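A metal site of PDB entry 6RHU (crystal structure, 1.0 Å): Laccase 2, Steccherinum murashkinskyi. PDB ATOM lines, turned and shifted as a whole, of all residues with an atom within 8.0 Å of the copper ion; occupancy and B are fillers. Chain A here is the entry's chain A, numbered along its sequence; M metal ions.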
ATOM      1  N   CYS A 208      11.803 -22.441  -1.199  1.00  0.00           N
ATOM      2  CA  CYS A 208      13.191 -22.788  -1.478  1.00  0.00           C
ATOM      3  C   CYS A 208      13.373 -23.530  -2.815  1.00  0.00           C
ATOM      4  O   CYS A 208      14.514 -23.712  -3.232  1.00  0.00           O
ATOM      5  CB  CYS A 208      13.793 -23.660  -0.408  1.00  0.00           C
ATOM      6  SG  CYS A 208      14.652 -22.632   0.827  1.00  0.00           S
ATOM      7  N   ASP A 209      12.297 -24.000  -3.434  1.00  0.00           N
ATOM      8  CA  ASP A 209      12.457 -24.825  -4.634  1.00  0.00           C
ATOM      9  C   ASP A 209      11.194 -24.844  -5.478  1.00  0.00           C
ATOM     10  O   ASP A 209      11.171 -24.217  -6.534  1.00  0.00           O
ATOM     11  CB  ASP A 209      13.026 -26.202  -4.290  1.00  0.00           C
ATOM     12  CG  ASP A 209      13.096 -27.174  -5.403  1.00  0.00           C
ATOM     13  OD1 ASP A 209      12.677 -26.905  -6.514  1.00  0.00           O
ATOM     14  OD2 ASP A 209      13.474 -28.339  -5.099  1.00  0.00           O
ATOM     15  N   PHE A 341      26.288 -26.280 -10.574  1.00  0.00           N
ATOM     16  CA  PHE A 341      25.867 -25.333 -11.575  1.00  0.00           C
ATOM     17  C   PHE A 341      27.030 -24.421 -11.912  1.00  0.00           C
ATOM     18  O   PHE A 341      27.912 -24.156 -11.111  1.00  0.00           O
ATOM     19  CB  PHE A 341      24.696 -24.510 -11.086  1.00  0.00           C
ATOM     20  CG  PHE A 341      23.410 -25.289 -11.003  1.00  0.00           C
ATOM     21  CD1 PHE A 341      23.011 -25.920  -9.847  1.00  0.00           C
ATOM     22  CD2 PHE A 341      22.604 -25.401 -12.123  1.00  0.00           C
ATOM     23  CE1 PHE A 341      21.849 -26.658  -9.802  1.00  0.00           C
ATOM     24  CE2 PHE A 341      21.421 -26.116 -12.052  1.00  0.00           C
ATOM     25  CZ  PHE A 341      21.059 -26.757 -10.910  1.00  0.00           C
ATOM     26  N   ALA A 392      19.705 -26.229 -18.527  1.00  0.00           N
ATOM     27  CA  ALA A 392      20.380 -26.846 -17.346  1.00  0.00           C
ATOM     28  C   ALA A 392      19.389 -27.676 -16.562  1.00  0.00           C
ATOM     29  O   ALA A 392      18.253 -27.213 -16.332  1.00  0.00           O
ATOM     30  CB  ALA A 392      20.970 -25.743 -16.472  1.00  0.00           C
ATOM     31  N   ALA A 393      19.830 -28.845 -16.067  1.00  0.00           N
ATOM     32  CA  ALA A 393      18.992 -29.732 -15.260  1.00  0.00           C
ATOM     33  C   ALA A 393      18.401 -28.990 -14.089  1.00  0.00           C
ATOM     34  O   ALA A 393      18.943 -27.975 -13.567  1.00  0.00           O
ATOM     35  CB  ALA A 393      19.868 -30.881 -14.802  1.00  0.00           C
ATOM     36  N   GLY A 394      17.287 -29.540 -13.598  1.00  0.00           N
ATOM     37  CA  GLY A 394      16.621 -29.030 -12.430  1.00  0.00           C
ATOM     38  C   GLY A 394      15.693 -27.876 -12.701  1.00  0.00           C
ATOM     39  O   GLY A 394      15.266 -27.235 -11.751  1.00  0.00           O
ATOM     40  N   GLY A 395      15.371 -27.611 -13.970  1.00  0.00           N
ATOM     41  CA  GLY A 395      14.501 -26.487 -14.301  1.00  0.00           C
ATOM     42  C   GLY A 395      13.043 -26.805 -13.961  1.00  0.00           C
ATOM     43  O   GLY A 395      12.680 -27.932 -13.595  1.00  0.00           O
ATOM     44  N   PRO A 396      12.156 -25.798 -14.101  1.00  0.00           N
ATOM     45  CA  PRO A 396      12.464 -24.465 -14.607  1.00  0.00           C
ATOM     46  C   PRO A 396      13.055 -23.597 -13.515  1.00  0.00           C
ATOM     47  O   PRO A 396      12.573 -23.513 -12.412  1.00  0.00           O
ATOM     48  CB  PRO A 396      11.094 -23.959 -15.083  1.00  0.00           C
ATOM     49  CG  PRO A 396      10.113 -24.665 -14.181  1.00  0.00           C
ATOM     50  CD  PRO A 396      10.727 -26.023 -13.959  1.00  0.00           C
ATOM     51  N   HIS A 397      14.151 -22.912 -13.895  1.00  0.00           N
ATOM     52  CA  HIS A 397      14.921 -22.101 -12.935  1.00  0.00           C
ATOM     53  C   HIS A 397      14.382 -20.692 -12.824  1.00  0.00           C
ATOM     54  O   HIS A 397      14.369 -19.979 -13.842  1.00  0.00           O
ATOM     55  CB  HIS A 397      16.381 -22.053 -13.331  1.00  0.00           C
ATOM     56  CG  HIS A 397      17.004 -23.390 -13.462  1.00  0.00           C
ATOM     57  ND1 HIS A 397      17.420 -24.101 -12.340  1.00  0.00           N
ATOM     58  CD2 HIS A 397      17.342 -24.091 -14.562  1.00  0.00           C
ATOM     59  CE1 HIS A 397      17.913 -25.236 -12.791  1.00  0.00           C
ATOM     60  NE2 HIS A 397      17.879 -25.275 -14.106  1.00  0.00           N
ATOM     61  N   PRO A 398      13.996 -20.240 -11.630  1.00  0.00           N
ATOM     62  CA  PRO A 398      13.552 -18.856 -11.446  1.00  0.00           C
ATOM     63  C   PRO A 398      14.742 -17.958 -11.132  1.00  0.00           C
ATOM     64  O   PRO A 398      15.223 -17.909 -10.000  1.00  0.00           O
ATOM     65  CB  PRO A 398      12.550 -18.955 -10.306  1.00  0.00           C
ATOM     66  CG  PRO A 398      13.109 -20.084  -9.441  1.00  0.00           C
ATOM     67  CD  PRO A 398      13.761 -21.033 -10.423  1.00  0.00           C
ATOM     68  N   PHE A 399      15.202 -17.197 -12.121  1.00  0.00           N
ATOM     69  CA  PHE A 399      16.335 -16.303 -11.918  1.00  0.00           C
ATOM     70  C   PHE A 399      15.897 -14.973 -11.347  1.00  0.00           C
ATOM     71  O   PHE A 399      14.894 -14.402 -11.755  1.00  0.00           O
ATOM     72  CB  PHE A 399      17.136 -16.112 -13.234  1.00  0.00           C
ATOM     73  CG  PHE A 399      18.273 -17.067 -13.361  1.00  0.00           C
ATOM     74  CD1 PHE A 399      18.059 -18.412 -13.588  1.00  0.00           C
ATOM     75  CD2 PHE A 399      19.585 -16.647 -13.131  1.00  0.00           C
ATOM     76  CE1 PHE A 399      19.114 -19.315 -13.557  1.00  0.00           C
ATOM     77  CE2 PHE A 399      20.646 -17.565 -13.094  1.00  0.00           C
ATOM     78  CZ  PHE A 399      20.409 -18.878 -13.333  1.00  0.00           C
ATOM     79  N   ILE A 430      13.096 -19.089 -16.338  1.00  0.00           N
ATOM     80  CA  ILE A 430      13.782 -19.132 -17.626  1.00  0.00           C
ATOM     81  C   ILE A 430      13.274 -20.272 -18.512  1.00  0.00           C
ATOM     82  O   ILE A 430      13.710 -20.416 -19.666  1.00  0.00           O
ATOM     83  CB  ILE A 430      15.287 -19.089 -17.513  1.00  0.00           C
ATOM     84  CG1 ILE A 430      15.850 -20.402 -16.931  1.00  0.00           C
ATOM     85  CG2 ILE A 430      15.719 -17.869 -16.689  1.00  0.00           C
ATOM     86  CD1 ILE A 430      17.369 -20.474 -17.027  1.00  0.00           C
ATOM     87  N   HIS A 452      21.015 -14.807  -9.517  1.00  0.00           N
ATOM     88  CA  HIS A 452      21.077 -16.214  -9.176  1.00  0.00           C
ATOM     89  C   HIS A 452      19.759 -16.895  -9.378  1.00  0.00           C
ATOM     90  O   HIS A 452      18.702 -16.282  -9.345  1.00  0.00           O
ATOM     91  CB  HIS A 452      21.584 -16.426  -7.730  1.00  0.00           C
ATOM     92  CG  HIS A 452      20.678 -15.867  -6.674  1.00  0.00           C
ATOM     93  ND1 HIS A 452      19.623 -16.571  -6.157  1.00  0.00           N
ATOM     94  CD2 HIS A 452      20.687 -14.682  -6.031  1.00  0.00           C
ATOM     95  CE1 HIS A 452      19.031 -15.814  -5.227  1.00  0.00           C
ATOM     96  NE2 HIS A 452      19.639 -14.647  -5.117  1.00  0.00           N
ATOM     97  N   CYS A 453      19.821 -18.233  -9.514  1.00  0.00           N
ATOM     98  CA  CYS A 453      18.595 -19.020  -9.435  1.00  0.00           C
ATOM     99  C   CYS A 453      18.083 -18.978  -8.002  1.00  0.00           C
ATOM    100  O   CYS A 453      18.868 -19.105  -7.053  1.00  0.00           O
ATOM    101  CB  CYS A 453      18.916 -20.483  -9.833  1.00  0.00           C
ATOM    102  SG  CYS A 453      17.366 -21.444  -9.786  1.00  0.00           S
ATOM    103  N   HIS A 454      16.773 -18.809  -7.835  1.00  0.00           N
ATOM    104  CA  HIS A 454      16.177 -18.728  -6.513  1.00  0.00           C
ATOM    105  C   HIS A 454      15.710 -20.079  -5.963  1.00  0.00           C
ATOM    106  O   HIS A 454      15.139 -20.101  -4.878  1.00  0.00           O
ATOM    107  CB  HIS A 454      15.037 -17.706  -6.505  1.00  0.00           C
ATOM    108  CG  HIS A 454      15.005 -16.909  -5.215  1.00  0.00           C
ATOM    109  ND1 HIS A 454      14.779 -17.452  -3.987  1.00  0.00           N
ATOM    110  CD2 HIS A 454      15.213 -15.585  -4.982  1.00  0.00           C
ATOM    111  CE1 HIS A 454      14.827 -16.474  -3.062  1.00  0.00           C
ATOM    112  NE2 HIS A 454      15.082 -15.312  -3.642  1.00  0.00           N
ATOM    113  N   ILE A 455      15.999 -21.173  -6.661  1.00  0.00           N
ATOM    114  CA  ILE A 455      15.922 -22.491  -6.030  1.00  0.00           C
ATOM    115  C   ILE A 455      17.162 -22.558  -5.141  1.00  0.00           C
ATOM    116  O   ILE A 455      18.307 -22.564  -5.645  1.00  0.00           O
ATOM    117  CB  ILE A 455      15.837 -23.606  -7.074  1.00  0.00           C
ATOM    118  CG1 ILE A 455      14.529 -23.492  -7.859  1.00  0.00           C
ATOM    119  CG2 ILE A 455      15.985 -24.970  -6.381  1.00  0.00           C
ATOM    120  CD1 ILE A 455      14.470 -24.348  -9.126  1.00  0.00           C
ATOM    121  N   ASP A 456      16.949 -22.531  -3.827  1.00  0.00           N
ATOM    122  CA  ASP A 456      18.073 -22.301  -2.943  1.00  0.00           C
ATOM    123  C   ASP A 456      19.121 -23.387  -3.011  1.00  0.00           C
ATOM    124  O   ASP A 456      20.322 -23.167  -2.827  1.00  0.00           O
ATOM    125  CB  ASP A 456      17.555 -22.087  -1.495  1.00  0.00           C
ATOM    126  CG  ASP A 456      18.386 -21.100  -0.676  1.00  0.00           C
ATOM    127  OD1 ASP A 456      18.896 -20.144  -1.310  1.00  0.00           O
ATOM    128  OD2 ASP A 456      18.445 -21.273   0.523  1.00  0.00           O
ATOM    129  N   TRP A 457      18.671 -24.630  -3.288  1.00  0.00           N
ATOM    130  CA  TRP A 457      19.582 -25.749  -3.448  1.00  0.00           C
ATOM    131  C   TRP A 457      20.524 -25.523  -4.641  1.00  0.00           C
ATOM    132  O   TRP A 457      21.663 -25.986  -4.647  1.00  0.00           O
ATOM    133  CB  TRP A 457      18.796 -27.064  -3.591  1.00  0.00           C
ATOM    134  CG  TRP A 457      17.687 -27.192  -2.564  1.00  0.00           C
ATOM    135  CD1 TRP A 457      16.353 -27.181  -2.817  1.00  0.00           C
ATOM    136  CD2 TRP A 457      17.830 -27.303  -1.163  1.00  0.00           C
ATOM    137  NE1 TRP A 457      15.655 -27.291  -1.662  1.00  0.00           N
ATOM    138  CE2 TRP A 457      16.523 -27.358  -0.613  1.00  0.00           C
ATOM    139  CE3 TRP A 457      18.905 -27.417  -0.296  1.00  0.00           C
ATOM    140  CZ2 TRP A 457      16.293 -27.492   0.730  1.00  0.00           C
ATOM    141  CZ3 TRP A 457      18.665 -27.511   1.025  1.00  0.00           C
ATOM    142  CH2 TRP A 457      17.375 -27.566   1.543  1.00  0.00           C
ATOM    143  N   HIS A 458      20.030 -24.825  -5.670  1.00  0.00           N
ATOM    144  CA  HIS A 458      20.823 -24.538  -6.854  1.00  0.00           C
ATOM    145  C   HIS A 458      21.792 -23.380  -6.609  1.00  0.00           C
ATOM    146  O   HIS A 458      22.927 -23.432  -7.081  1.00  0.00           O
ATOM    147  CB  HIS A 458      19.906 -24.213  -8.042  1.00  0.00           C
ATOM    148  CG  HIS A 458      19.009 -25.322  -8.444  1.00  0.00           C
ATOM    149  ND1 HIS A 458      18.082 -25.155  -9.460  1.00  0.00           N
ATOM    150  CD2 HIS A 458      18.922 -26.588  -7.955  1.00  0.00           C
ATOM    151  CE1 HIS A 458      17.464 -26.321  -9.559  1.00  0.00           C
ATOM    152  NE2 HIS A 458      17.933 -27.205  -8.690  1.00  0.00           N
ATOM    153  N   LEU A 459      21.350 -22.347  -5.885  1.00  0.00           N
ATOM    154  CA  LEU A 459      22.271 -21.304  -5.457  1.00  0.00           C
ATOM    155  C   LEU A 459      23.412 -21.908  -4.674  1.00  0.00           C
ATOM    156  O   LEU A 459      24.604 -21.591  -4.929  1.00  0.00           O
ATOM    157  CB  LEU A 459      21.519 -20.277  -4.648  1.00  0.00           C
ATOM    158  CG  LEU A 459      22.383 -19.216  -3.938  1.00  0.00           C
ATOM    159  CD1 LEU A 459      23.266 -18.463  -4.907  1.00  0.00           C
ATOM    160  CD2 LEU A 459      21.541 -18.279  -3.113  1.00  0.00           C
ATOM    161  N   PHE A 463      24.809 -21.707  -8.693  1.00  0.00           N
ATOM    162  CA  PHE A 463      24.113 -21.127  -9.870  1.00  0.00           C
ATOM    163  C   PHE A 463      23.919 -19.626  -9.674  1.00  0.00           C
ATOM    164  O   PHE A 463      22.803 -19.140  -9.430  1.00  0.00           O
ATOM    165  CB  PHE A 463      22.808 -21.848 -10.112  1.00  0.00           C
ATOM    166  CG  PHE A 463      22.343 -21.943 -11.540  1.00  0.00           C
ATOM    167  CD1 PHE A 463      23.163 -21.675 -12.617  1.00  0.00           C
ATOM    168  CD2 PHE A 463      21.071 -22.425 -11.796  1.00  0.00           C
ATOM    169  CE1 PHE A 463      22.707 -21.916 -13.913  1.00  0.00           C
ATOM    170  CE2 PHE A 463      20.615 -22.667 -13.092  1.00  0.00           C
ATOM    171  CZ  PHE A 463      21.437 -22.436 -14.145  1.00  0.00           C
HETATM  172 CU    CU M   1      17.685 -23.480 -10.435  1.00  0.00          CU
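Ile 455 touches the copper ion (CD1 to CU, 3.6 Å). Phe 463 touches the copper ion (CD2 to CU, 3.8 Å). Of the 21 residues printed, 5 come within 4 Å of the copper ion. Along chain A the residues within 4 Å of the copper ion span positions 397 to 463.
The copper ion is bound by a ring nitrogen (ND1) of His 458 (2.0 Å), a ring nitrogen (ND1) of His 397 (2.0 Å) and the side-chain sulfur of Cys 453 (2.2 Å). The copper ion has three donor atoms within binding distance.
The backbone carbonyl oxygen (O) of His 458 lies within hydrogen-bond range of the backbone NH (N) of Phe 463 (3.0 Å). O of Ala 393 sits at hydrogen-bond distance from NE2 of His 397 (3.0 Å). A ring nitrogen (NE2) of His 397 is in hydrogen-bond range of the backbone NH of Gly 395, 3.4 Å away. The backbone carbonyl oxygen of Ala 392 lies within hydrogen-bond range of a ring nitrogen (NE2) of His 397, 3.0 Å away. The backbone carbonyl oxygen (O) of His 397 lies within hydrogen-bond range of the backbone NH (N) of Ile 430 (2.9 Å). The side-chain sulfur (SG) of Cys 453 sits close to the backbone NH (N) of Ile 455 (3.4 Å). The backbone NH (N) of Cys 453 is in hydrogen-bond range of the backbone carbonyl oxygen (O) of Phe 463, 3.1 Å away.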
